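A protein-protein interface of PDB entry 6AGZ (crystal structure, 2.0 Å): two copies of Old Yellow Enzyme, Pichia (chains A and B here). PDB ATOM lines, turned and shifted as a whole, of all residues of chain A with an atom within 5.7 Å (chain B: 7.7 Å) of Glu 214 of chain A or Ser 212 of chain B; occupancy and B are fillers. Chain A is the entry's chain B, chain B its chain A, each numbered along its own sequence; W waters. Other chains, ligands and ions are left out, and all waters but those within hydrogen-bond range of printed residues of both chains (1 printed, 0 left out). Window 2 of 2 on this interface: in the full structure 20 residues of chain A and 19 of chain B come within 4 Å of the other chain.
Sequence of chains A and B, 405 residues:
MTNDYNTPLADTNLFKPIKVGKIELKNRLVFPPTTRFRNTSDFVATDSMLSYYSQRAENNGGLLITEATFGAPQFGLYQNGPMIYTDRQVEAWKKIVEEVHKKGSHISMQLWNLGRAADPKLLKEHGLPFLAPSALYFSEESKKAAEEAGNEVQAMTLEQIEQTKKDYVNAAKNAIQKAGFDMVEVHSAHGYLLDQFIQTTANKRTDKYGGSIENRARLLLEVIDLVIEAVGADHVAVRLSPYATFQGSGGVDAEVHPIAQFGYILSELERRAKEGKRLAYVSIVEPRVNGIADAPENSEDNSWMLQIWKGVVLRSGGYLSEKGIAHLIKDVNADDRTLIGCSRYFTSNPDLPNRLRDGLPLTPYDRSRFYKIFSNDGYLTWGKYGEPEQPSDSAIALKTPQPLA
N of Ile 213 of chain B sits at hydrogen-bond distance from OE2 of Glu 214 of chain A (2.9 Å).
OE2 of Glu 214 of chain B is in hydrogen-bond range of N of Ile 213 of chain A (2.9 Å).
OE1 of Glu 214 of chain A sits close to OE1 of Glu 214 of chain B, 2.9 Å away.
Water W1 lies within hydrogen-bond range of NH2 of Arg 216 of chain A (2.9 Å), OE2 of Glu 214 of chain B (3.1 Å) and N of Ile 213 of chain A (3.4 Å).
The side-chain carboxylate of Glu 214 of chain B sits at hydrogen-bond distance from the side-chain hydroxyl of Ser 212 of chain B (3.5 Å).
The side-chain hydroxyl (OG) of Ser 212 of chain B lies within hydrogen-bond range of the backbone NH (N) of Asn 215 of chain B (3.0 Å).
The backbone carbonyl oxygen (O) of Ile 213 of chain B lies within hydrogen-bond range of the side-chain amide nitrogen (NE2) of Gln 261 of chain B, at 2.9 Å.
OG of Ser 212 of chain A sits close to N of Glu 214 of chain A.
The side-chain hydroxyl (OG) of Ser 212 of chain A sits at hydrogen-bond distance from the backbone NH (N) of Asn 215 of chain A (2.9 Å).
NE2 of Gln 261 of chain A sits at hydrogen-bond distance from O of Ile 213 of chain A, 2.9 Å away.
Printed residues of chain A that touch a printed residue of chain B: Ser 212, Ile 213, Glu 214 and Tyr 264.
Hydrophobic or aromatic side chains of chain A within 4 Å of the printed part of chain B: Ile 213 and Tyr 264.
Hydrophobic or aromatic side chains of chain B within 4 Å of the printed part of chain A: Ile 213 and Tyr 264.
Among the printed residues, 7 pairs touch across the chains.
Among the printed residues, merely in contact across the chains: Ser 212 of chain A with Glu 214 of chain B (3.6 Å), Ile 213 of chain A with Tyr 264 of chain B (3.7 Å), Glu 214 of chain A with Ser 212 of chain B (3.5 Å) and Tyr 264 of chain A with Ile 213 of chain B (3.8 Å).
Ser 212 of chain A touches Glu 214 of chain B, and with the chains exchanged Glu 214 of chain A touches Ser 212 of chain B.
Ile 213 of chain A touches Glu 214 of chain B, and with the chains exchanged Glu 214 of chain A touches Ile 213 of chain B.
Ile 213 of chain A touches Tyr 264 of chain B, and with the chains exchanged Tyr 264 of chain A touches Ile 213 of chain B.
Glu 214 of chain B touches its own counterpart, Glu 214 of chain A.
Printed residues of chain B within 4 Å of Ser 212 of chain A: Glu 214 (3.6 Å).
Of the printed residues of chain B, Ile 213 of chain A touches Glu 214 and Tyr 264.
Glu 214 of chain A touches three residues of chain B.
Printed residues of chain B within 4 Å of Tyr 264 of chain A: Ile 213.
Ser 212 of chain B touches one residue of chain A.
Of the printed residues of chain A, Ile 213 of chain B touches Glu 214 (2.9 Å) and Tyr 264 (3.8 Å).
Printed residues of chain A within 4 Å of Glu 214 of chain B: Ser 212, Ile 213 and Glu 214.
The nearest residue of chain B that does not touch Glu 214 of chain A is Arg 216 of chain B (4.9 Å).
The nearest printed residue of chain A that does not touch Ser 212 of chain B is Ser 212 of chain A (6.4 Å).
The nearest printed residue of chain B that does not touch Ser 212 of chain A is Ser 212 of chain B (6.4 Å).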
ATOM      1  N   LYS A 208      -9.307 -17.634 -29.276  1.00  0.00           N
ATOM      2  CA  LYS A 208     -10.749 -17.924 -29.249  1.00  0.00           C
ATOM      3  C   LYS A 208     -11.131 -19.118 -30.116  1.00  0.00           C
ATOM      4  O   LYS A 208     -12.200 -19.712 -29.916  1.00  0.00           O
ATOM      5  CB  LYS A 208     -11.601 -16.735 -29.741  1.00  0.00           C
ATOM      6  CG  LYS A 208     -11.173 -15.299 -29.453  1.00  0.00           C
ATOM      7  CD  LYS A 208     -10.862 -15.047 -27.994  1.00  0.00           C
ATOM      8  CE  LYS A 208      -9.973 -13.813 -27.805  1.00  0.00           C
ATOM      9  NZ  LYS A 208      -8.515 -13.997 -28.084  1.00  0.00           N
ATOM     10  N   SER A 212     -10.556 -25.793 -26.963  1.00  0.00           N
ATOM     11  CA  SER A 212     -11.748 -26.284 -26.284  1.00  0.00           C
ATOM     12  C   SER A 212     -12.747 -26.732 -27.339  1.00  0.00           C
ATOM     13  O   SER A 212     -12.609 -26.423 -28.526  1.00  0.00           O
ATOM     14  CB  SER A 212     -12.367 -25.220 -25.369  1.00  0.00           C
ATOM     15  OG  SER A 212     -13.140 -24.293 -26.110  1.00  0.00           O
ATOM     16  N   ILE A 213     -13.759 -27.473 -26.885  1.00  0.00           N
ATOM     17  CA  ILE A 213     -14.820 -27.919 -27.783  1.00  0.00           C
ATOM     18  C   ILE A 213     -15.530 -26.720 -28.399  1.00  0.00           C
ATOM     19  O   ILE A 213     -15.744 -26.655 -29.615  1.00  0.00           O
ATOM     20  CB  ILE A 213     -15.806 -28.832 -27.035  1.00  0.00           C
ATOM     21  CG1 ILE A 213     -15.151 -30.171 -26.695  1.00  0.00           C
ATOM     22  CG2 ILE A 213     -17.053 -29.048 -27.864  1.00  0.00           C
ATOM     23  CD1 ILE A 213     -16.016 -31.069 -25.837  1.00  0.00           C
ATOM     24  N   GLU A 214     -15.904 -25.748 -27.563  1.00  0.00           N
ATOM     25  CA  GLU A 214     -16.598 -24.566 -28.065  1.00  0.00           C
ATOM     26  C   GLU A 214     -15.690 -23.723 -28.950  1.00  0.00           C
ATOM     27  O   GLU A 214     -16.152 -23.124 -29.928  1.00  0.00           O
ATOM     28  CB  GLU A 214     -17.131 -23.732 -26.898  1.00  0.00           C
ATOM     29  CG  GLU A 214     -18.158 -24.439 -26.020  1.00  0.00           C
ATOM     30  CD  GLU A 214     -17.527 -25.331 -24.965  1.00  0.00           C
ATOM     31  OE1 GLU A 214     -16.288 -25.496 -24.979  1.00  0.00           O
ATOM     32  OE2 GLU A 214     -18.273 -25.866 -24.117  1.00  0.00           O
ATOM     33  N   ASN A 215     -14.395 -23.669 -28.629  1.00  0.00           N
ATOM     34  CA  ASN A 215     -13.478 -22.829 -29.393  1.00  0.00           C
ATOM     35  C   ASN A 215     -13.158 -23.440 -30.752  1.00  0.00           C
ATOM     36  O   ASN A 215     -13.039 -22.717 -31.749  1.00  0.00           O
ATOM     37  CB  ASN A 215     -12.195 -22.590 -28.598  1.00  0.00           C
ATOM     38  CG  ASN A 215     -12.400 -21.639 -27.437  1.00  0.00           C
ATOM     39  OD1 ASN A 215     -13.445 -20.999 -27.322  1.00  0.00           O
ATOM     40  ND2 ASN A 215     -11.397 -21.534 -26.573  1.00  0.00           N
ATOM     41  N   ARG A 216     -13.009 -24.764 -30.815  1.00  0.00           N
ATOM     42  CA  ARG A 216     -12.702 -25.404 -32.090  1.00  0.00           C
ATOM     43  C   ARG A 216     -13.889 -25.361 -33.042  1.00  0.00           C
ATOM     44  O   ARG A 216     -13.702 -25.298 -34.263  1.00  0.00           O
ATOM     45  CB  ARG A 216     -12.254 -26.847 -31.863  1.00  0.00           C
ATOM     46  CG  ARG A 216     -10.839 -26.974 -31.326  1.00  0.00           C
ATOM     47  CD  ARG A 216     -10.406 -28.426 -31.255  1.00  0.00           C
ATOM     48  NE  ARG A 216     -11.217 -29.185 -30.308  1.00  0.00           N
ATOM     49  CZ  ARG A 216     -10.943 -29.290 -29.011  1.00  0.00           C
ATOM     50  NH1 ARG A 216      -9.874 -28.689 -28.506  1.00  0.00           N
ATOM     51  NH2 ARG A 216     -11.734 -30.003 -28.220  1.00  0.00           N
ATOM     52  N   ALA A 217     -15.108 -25.393 -32.512  1.00  0.00           N
ATOM     53  CA  ALA A 217     -16.306 -25.296 -33.335  1.00  0.00           C
ATOM     54  C   ALA A 217     -16.700 -23.858 -33.644  1.00  0.00           C
ATOM     55  O   ALA A 217     -17.701 -23.646 -34.337  1.00  0.00           O
ATOM     56  CB  ALA A 217     -17.473 -26.008 -32.646  1.00  0.00           C
ATOM     57  N   ARG A 218     -15.934 -22.876 -33.165  1.00  0.00           N
ATOM     58  CA  ARG A 218     -16.383 -21.488 -33.222  1.00  0.00           C
ATOM     59  C   ARG A 218     -16.458 -20.976 -34.655  1.00  0.00           C
ATOM     60  O   ARG A 218     -17.443 -20.337 -35.041  1.00  0.00           O
ATOM     61  CB  ARG A 218     -15.463 -20.599 -32.387  1.00  0.00           C
ATOM     62  CG  ARG A 218     -15.913 -19.148 -32.346  1.00  0.00           C
ATOM     63  CD  ARG A 218     -15.091 -18.334 -31.364  1.00  0.00           C
ATOM     64  NE  ARG A 218     -15.008 -18.977 -30.056  1.00  0.00           N
ATOM     65  CZ  ARG A 218     -15.974 -18.951 -29.144  1.00  0.00           C
ATOM     66  NH1 ARG A 218     -17.111 -18.311 -29.392  1.00  0.00           N
ATOM     67  NH2 ARG A 218     -15.805 -19.566 -27.982  1.00  0.00           N
ATOM     68  N   GLN A 261     -17.278 -33.493 -29.425  1.00  0.00           N
ATOM     69  CA  GLN A 261     -17.056 -32.296 -30.230  1.00  0.00           C
ATOM     70  C   GLN A 261     -18.190 -32.086 -31.228  1.00  0.00           C
ATOM     71  O   GLN A 261     -18.916 -31.081 -31.172  1.00  0.00           O
ATOM     72  CB  GLN A 261     -15.710 -32.418 -30.950  1.00  0.00           C
ATOM     73  CG  GLN A 261     -15.377 -31.268 -31.876  1.00  0.00           C
ATOM     74  CD  GLN A 261     -15.054 -29.997 -31.124  1.00  0.00           C
ATOM     75  OE1 GLN A 261     -14.104 -29.950 -30.344  1.00  0.00           O
ATOM     76  NE2 GLN A 261     -15.848 -28.958 -31.351  1.00  0.00           N
ATOM     77  N   TYR A 264     -21.418 -31.466 -29.639  1.00  0.00           N
ATOM     78  CA  TYR A 264     -21.644 -30.056 -29.341  1.00  0.00           C
ATOM     79  C   TYR A 264     -22.074 -29.292 -30.586  1.00  0.00           C
ATOM     80  O   TYR A 264     -22.974 -28.448 -30.521  1.00  0.00           O
ATOM     81  CB  TYR A 264     -20.387 -29.427 -28.746  1.00  0.00           C
ATOM     82  CG  TYR A 264     -20.449 -27.915 -28.654  1.00  0.00           C
ATOM     83  CD1 TYR A 264     -21.130 -27.290 -27.618  1.00  0.00           C
ATOM     84  CD2 TYR A 264     -19.829 -27.114 -29.607  1.00  0.00           C
ATOM     85  CE1 TYR A 264     -21.192 -25.912 -27.531  1.00  0.00           C
ATOM     86  CE2 TYR A 264     -19.886 -25.734 -29.528  1.00  0.00           C
ATOM     87  CZ  TYR A 264     -20.568 -25.140 -28.487  1.00  0.00           C
ATOM     88  OH  TYR A 264     -20.627 -23.767 -28.405  1.00  0.00           O
ATOM     89  N   PHE B 197     -23.365 -29.424 -10.850  1.00  0.00           N
ATOM     90  CA  PHE B 197     -22.274 -28.736 -11.531  1.00  0.00           C
ATOM     91  C   PHE B 197     -22.233 -29.081 -13.013  1.00  0.00           C
ATOM     92  O   PHE B 197     -21.834 -28.244 -13.831  1.00  0.00           O
ATOM     93  CB  PHE B 197     -20.937 -29.066 -10.867  1.00  0.00           C
ATOM     94  CG  PHE B 197     -20.583 -28.144  -9.737  1.00  0.00           C
ATOM     95  CD1 PHE B 197     -21.073 -28.369  -8.461  1.00  0.00           C
ATOM     96  CD2 PHE B 197     -19.770 -27.043  -9.952  1.00  0.00           C
ATOM     97  CE1 PHE B 197     -20.754 -27.516  -7.420  1.00  0.00           C
ATOM     98  CE2 PHE B 197     -19.447 -26.186  -8.917  1.00  0.00           C
ATOM     99  CZ  PHE B 197     -19.942 -26.423  -7.648  1.00  0.00           C
ATOM    100  N   ILE B 198     -22.651 -30.295 -13.379  1.00  0.00           N
ATOM    101  CA  ILE B 198     -22.629 -30.686 -14.786  1.00  0.00           C
ATOM    102  C   ILE B 198     -23.766 -30.028 -15.565  1.00  0.00           C
ATOM    103  O   ILE B 198     -23.597 -29.671 -16.738  1.00  0.00           O
ATOM    104  CB  ILE B 198     -22.680 -32.221 -14.901  1.00  0.00           C
ATOM    105  CG1 ILE B 198     -21.452 -32.850 -14.242  1.00  0.00           C
ATOM    106  CG2 ILE B 198     -22.773 -32.656 -16.353  1.00  0.00           C
ATOM    107  CD1 ILE B 198     -21.513 -34.360 -14.166  1.00  0.00           C
ATOM    108  N   THR B 200     -26.538 -27.572 -17.144  1.00  0.00           N
ATOM    109  CA  THR B 200     -26.746 -26.163 -17.462  1.00  0.00           C
ATOM    110  C   THR B 200     -27.919 -25.581 -16.686  1.00  0.00           C
ATOM    111  O   THR B 200     -27.919 -24.387 -16.362  1.00  0.00           O
ATOM    112  CB  THR B 200     -26.979 -25.983 -18.964  1.00  0.00           C
ATOM    113  OG1 THR B 200     -28.064 -26.820 -19.386  1.00  0.00           O
ATOM    114  CG2 THR B 200     -25.728 -26.346 -19.751  1.00  0.00           C
ATOM    115  N   ASN B 203     -26.208 -24.908 -13.142  1.00  0.00           N
ATOM    116  CA  ASN B 203     -24.911 -24.244 -13.058  1.00  0.00           C
ATOM    117  C   ASN B 203     -24.933 -22.987 -13.923  1.00  0.00           C
ATOM    118  O   ASN B 203     -24.864 -23.072 -15.154  1.00  0.00           O
ATOM    119  CB  ASN B 203     -23.792 -25.192 -13.491  1.00  0.00           C
ATOM    120  CG  ASN B 203     -22.407 -24.636 -13.207  1.00  0.00           C
ATOM    121  OD1 ASN B 203     -22.240 -23.444 -12.955  1.00  0.00           O
ATOM    122  ND2 ASN B 203     -21.402 -25.506 -13.244  1.00  0.00           N
ATOM    123  N   ARG B 205     -22.603 -20.582 -13.047  1.00  0.00           N
ATOM    124  CA  ARG B 205     -21.353 -19.976 -12.612  1.00  0.00           C
ATOM    125  C   ARG B 205     -20.590 -19.393 -13.795  1.00  0.00           C
ATOM    126  O   ARG B 205     -20.661 -19.893 -14.921  1.00  0.00           O
ATOM    127  CB  ARG B 205     -20.482 -21.006 -11.890  1.00  0.00           C
ATOM    128  CG  ARG B 205     -21.120 -21.601 -10.646  1.00  0.00           C
ATOM    129  CD  ARG B 205     -20.204 -22.619  -9.985  1.00  0.00           C
ATOM    130  NE  ARG B 205     -19.078 -21.983  -9.308  1.00  0.00           N
ATOM    131  CZ  ARG B 205     -19.092 -21.603  -8.035  1.00  0.00           C
ATOM    132  NH1 ARG B 205     -20.177 -21.798  -7.297  1.00  0.00           N
ATOM    133  NH2 ARG B 205     -18.023 -21.029  -7.498  1.00  0.00           N
ATOM    134  N   ASP B 207     -17.153 -18.533 -13.253  1.00  0.00           N
ATOM    135  CA  ASP B 207     -15.750 -18.856 -13.044  1.00  0.00           C
ATOM    136  C   ASP B 207     -15.426 -20.139 -13.811  1.00  0.00           C
ATOM    137  O   ASP B 207     -16.197 -20.590 -14.661  1.00  0.00           O
ATOM    138  CB  ASP B 207     -15.426 -18.952 -11.551  1.00  0.00           C
ATOM    139  CG  ASP B 207     -16.243 -20.013 -10.823  1.00  0.00           C
ATOM    140  OD1 ASP B 207     -16.905 -20.845 -11.479  1.00  0.00           O
ATOM    141  OD2 ASP B 207     -16.211 -20.015  -9.575  1.00  0.00           O
ATOM    142  N   LYS B 208     -14.272 -20.741 -13.525  1.00  0.00           N
ATOM    143  CA  LYS B 208     -13.843 -21.912 -14.282  1.00  0.00           C
ATOM    144  C   LYS B 208     -14.641 -23.173 -13.963  1.00  0.00           C
ATOM    145  O   LYS B 208     -14.337 -24.227 -14.531  1.00  0.00           O
ATOM    146  CB  LYS B 208     -12.353 -22.173 -14.049  1.00  0.00           C
ATOM    147  CG  LYS B 208     -12.007 -22.652 -12.652  1.00  0.00           C
ATOM    148  CD  LYS B 208     -10.581 -23.177 -12.611  1.00  0.00           C
ATOM    149  CE  LYS B 208     -10.176 -23.609 -11.212  1.00  0.00           C
ATOM    150  NZ  LYS B 208      -8.808 -24.200 -11.205  1.00  0.00           N
ATOM    151  N   TYR B 209     -15.642 -23.110 -13.086  1.00  0.00           N
ATOM    152  CA  TYR B 209     -16.477 -24.265 -12.787  1.00  0.00           C
ATOM    153  C   TYR B 209     -17.842 -24.192 -13.459  1.00  0.00           C
ATOM    154  O   TYR B 209     -18.713 -25.016 -13.165  1.00  0.00           O
ATOM    155  CB  TYR B 209     -16.634 -24.429 -11.274  1.00  0.00           C
ATOM    156  CG  TYR B 209     -15.371 -24.912 -10.596  1.00  0.00           C
ATOM    157  CD1 TYR B 209     -15.002 -26.250 -10.649  1.00  0.00           C
ATOM    158  CD2 TYR B 209     -14.544 -24.030  -9.913  1.00  0.00           C
ATOM    159  CE1 TYR B 209     -13.845 -26.698 -10.037  1.00  0.00           C
ATOM    160  CE2 TYR B 209     -13.386 -24.469  -9.296  1.00  0.00           C
ATOM    161  CZ  TYR B 209     -13.042 -25.804  -9.361  1.00  0.00           C
ATOM    162  OH  TYR B 209     -11.891 -26.245  -8.750  1.00  0.00           O
ATOM    163  N   GLY B 210     -18.047 -23.223 -14.353  1.00  0.00           N
ATOM    164  CA  GLY B 210     -19.267 -23.138 -15.127  1.00  0.00           C
ATOM    165  C   GLY B 210     -19.029 -22.347 -16.396  1.00  0.00           C
ATOM    166  O   GLY B 210     -17.975 -21.738 -16.586  1.00  0.00           O
ATOM    167  N   GLY B 211     -20.034 -22.362 -17.269  1.00  0.00           N
ATOM    168  CA  GLY B 211     -19.995 -21.593 -18.494  1.00  0.00           C
ATOM    169  C   GLY B 211     -19.517 -22.333 -19.723  1.00  0.00           C
ATOM    170  O   GLY B 211     -19.518 -21.748 -20.813  1.00  0.00           O
ATOM    171  N   SER B 212     -19.106 -23.591 -19.591  1.00  0.00           N
ATOM    172  CA  SER B 212     -18.730 -24.394 -20.747  1.00  0.00           C
ATOM    173  C   SER B 212     -18.810 -25.860 -20.356  1.00  0.00           C
ATOM    174  O   SER B 212     -19.009 -26.203 -19.187  1.00  0.00           O
ATOM    175  CB  SER B 212     -17.329 -24.036 -21.256  1.00  0.00           C
ATOM    176  OG  SER B 212     -16.325 -24.514 -20.379  1.00  0.00           O
ATOM    177  N   ILE B 213     -18.660 -26.728 -21.359  1.00  0.00           N
ATOM    178  CA  ILE B 213     -18.652 -28.164 -21.096  1.00  0.00           C
ATOM    179  C   ILE B 213     -17.467 -28.532 -20.212  1.00  0.00           C
ATOM    180  O   ILE B 213     -17.614 -29.237 -19.207  1.00  0.00           O
ATOM    181  CB  ILE B 213     -18.633 -28.950 -22.417  1.00  0.00           C
ATOM    182  CG1 ILE B 213     -19.892 -28.654 -23.232  1.00  0.00           C
ATOM    183  CG2 ILE B 213     -18.511 -30.437 -22.146  1.00  0.00           C
ATOM    184  CD1 ILE B 213     -19.880 -29.285 -24.600  1.00  0.00           C
ATOM    185  N   GLU B 214     -16.274 -28.057 -20.578  1.00  0.00           N
ATOM    186  CA  GLU B 214     -15.085 -28.333 -19.777  1.00  0.00           C
ATOM    187  C   GLU B 214     -15.234 -27.785 -18.362  1.00  0.00           C
ATOM    188  O   GLU B 214     -14.830 -28.435 -17.391  1.00  0.00           O
ATOM    189  CB  GLU B 214     -13.847 -27.739 -20.451  1.00  0.00           C
ATOM    190  CG  GLU B 214     -13.513 -28.330 -21.819  1.00  0.00           C
ATOM    191  CD  GLU B 214     -14.349 -27.748 -22.947  1.00  0.00           C
ATOM    192  OE1 GLU B 214     -15.224 -26.899 -22.674  1.00  0.00           O
ATOM    193  OE2 GLU B 214     -14.124 -28.138 -24.112  1.00  0.00           O
ATOM    194  N   ASN B 215     -15.817 -26.592 -18.225  1.00  0.00           N
ATOM    195  CA  ASN B 215     -15.947 -25.976 -16.909  1.00  0.00           C
ATOM    196  C   ASN B 215     -16.998 -26.680 -16.061  1.00  0.00           C
ATOM    197  O   ASN B 215     -16.807 -26.859 -14.852  1.00  0.00           O
ATOM    198  CB  ASN B 215     -16.280 -24.494 -17.059  1.00  0.00           C
ATOM    199  CG  ASN B 215     -15.104 -23.682 -17.561  1.00  0.00           C
ATOM    200  OD1 ASN B 215     -14.054 -24.232 -17.896  1.00  0.00           O
ATOM    201  ND2 ASN B 215     -15.273 -22.367 -17.618  1.00  0.00           N
ATOM    202  N   ARG B 216     -18.119 -27.078 -16.668  1.00  0.00           N
ATOM    203  CA  ARG B 216     -19.167 -27.749 -15.903  1.00  0.00           C
ATOM    204  C   ARG B 216     -18.729 -29.132 -15.438  1.00  0.00           C
ATOM    205  O   ARG B 216     -19.163 -29.592 -14.377  1.00  0.00           O
ATOM    206  CB  ARG B 216     -20.448 -27.849 -16.731  1.00  0.00           C
ATOM    207  CG  ARG B 216     -21.225 -26.547 -16.825  1.00  0.00           C
ATOM    208  CD  ARG B 216     -22.544 -26.741 -17.554  1.00  0.00           C
ATOM    209  NE  ARG B 216     -22.349 -27.105 -18.953  1.00  0.00           N
ATOM    210  CZ  ARG B 216     -22.277 -26.226 -19.948  1.00  0.00           C
ATOM    211  NH1 ARG B 216     -22.098 -26.643 -21.194  1.00  0.00           N
ATOM    212  NH2 ARG B 216     -22.387 -24.929 -19.695  1.00  0.00           N
ATOM    213  N   ALA B 217     -17.878 -29.803 -16.208  1.00  0.00           N
ATOM    214  CA  ALA B 217     -17.352 -31.107 -15.834  1.00  0.00           C
ATOM    215  C   ALA B 217     -16.107 -31.015 -14.965  1.00  0.00           C
ATOM    216  O   ALA B 217     -15.581 -32.054 -14.549  1.00  0.00           O
ATOM    217  CB  ALA B 217     -17.035 -31.928 -17.088  1.00  0.00           C
ATOM    218  N   ARG B 218     -15.632 -29.801 -14.674  1.00  0.00           N
ATOM    219  CA  ARG B 218     -14.326 -29.644 -14.042  1.00  0.00           C
ATOM    220  C   ARG B 218     -14.313 -30.207 -12.626  1.00  0.00           C
ATOM    221  O   ARG B 218     -13.375 -30.913 -12.243  1.00  0.00           O
ATOM    222  CB  ARG B 218     -13.916 -28.171 -14.036  1.00  0.00           C
ATOM    223  CG  ARG B 218     -12.522 -27.940 -13.480  1.00  0.00           C
ATOM    224  CD  ARG B 218     -12.069 -26.505 -13.679  1.00  0.00           C
ATOM    225  NE  ARG B 218     -12.342 -26.030 -15.032  1.00  0.00           N
ATOM    226  CZ  ARG B 218     -11.594 -26.318 -16.092  1.00  0.00           C
ATOM    227  NH1 ARG B 218     -10.521 -27.087 -15.962  1.00  0.00           N
ATOM    228  NH2 ARG B 218     -11.920 -25.838 -17.284  1.00  0.00           N
ATOM    229  N   VAL B 256     -27.377 -27.354 -23.667  1.00  0.00           N
ATOM    230  CA  VAL B 256     -26.358 -28.124 -24.367  1.00  0.00           C
ATOM    231  C   VAL B 256     -26.691 -29.597 -24.183  1.00  0.00           C
ATOM    232  O   VAL B 256     -26.900 -30.052 -23.052  1.00  0.00           O
ATOM    233  CB  VAL B 256     -24.945 -27.802 -23.848  1.00  0.00           C
ATOM    234  CG1 VAL B 256     -23.910 -28.667 -24.553  1.00  0.00           C
ATOM    235  CG2 VAL B 256     -24.629 -26.328 -24.049  1.00  0.00           C
ATOM    236  N   GLN B 261     -22.012 -32.944 -23.416  1.00  0.00           N
ATOM    237  CA  GLN B 261     -21.464 -32.739 -22.077  1.00  0.00           C
ATOM    238  C   GLN B 261     -20.918 -34.042 -21.500  1.00  0.00           C
ATOM    239  O   GLN B 261     -19.717 -34.171 -21.218  1.00  0.00           O
ATOM    240  CB  GLN B 261     -22.560 -32.157 -21.181  1.00  0.00           C
ATOM    241  CG  GLN B 261     -22.153 -31.859 -19.755  1.00  0.00           C
ATOM    242  CD  GLN B 261     -21.226 -30.668 -19.641  1.00  0.00           C
ATOM    243  OE1 GLN B 261     -21.620 -29.530 -19.900  1.00  0.00           O
ATOM    244  NE2 GLN B 261     -19.990 -30.922 -19.233  1.00  0.00           N
ATOM    245  N   TYR B 264     -18.150 -35.575 -23.416  1.00  0.00           N
ATOM    246  CA  TYR B 264     -16.846 -35.049 -23.032  1.00  0.00           C
ATOM    247  C   TYR B 264     -16.362 -35.672 -21.730  1.00  0.00           C
ATOM    248  O   TYR B 264     -15.174 -35.990 -21.597  1.00  0.00           O
ATOM    249  CB  TYR B 264     -16.901 -33.527 -22.908  1.00  0.00           C
ATOM    250  CG  TYR B 264     -15.713 -32.930 -22.181  1.00  0.00           C
ATOM    251  CD1 TYR B 264     -14.517 -32.685 -22.844  1.00  0.00           C
ATOM    252  CD2 TYR B 264     -15.787 -32.611 -20.830  1.00  0.00           C
ATOM    253  CE1 TYR B 264     -13.429 -32.143 -22.182  1.00  0.00           C
ATOM    254  CE2 TYR B 264     -14.707 -32.071 -20.161  1.00  0.00           C
ATOM    255  CZ  TYR B 264     -13.531 -31.837 -20.840  1.00  0.00           C
ATOM    256  OH  TYR B 264     -12.456 -31.299 -20.174  1.00  0.00           O
HETATM  257  O   HOH W   1     -11.807 -29.740 -25.363  1.00  0.00           O
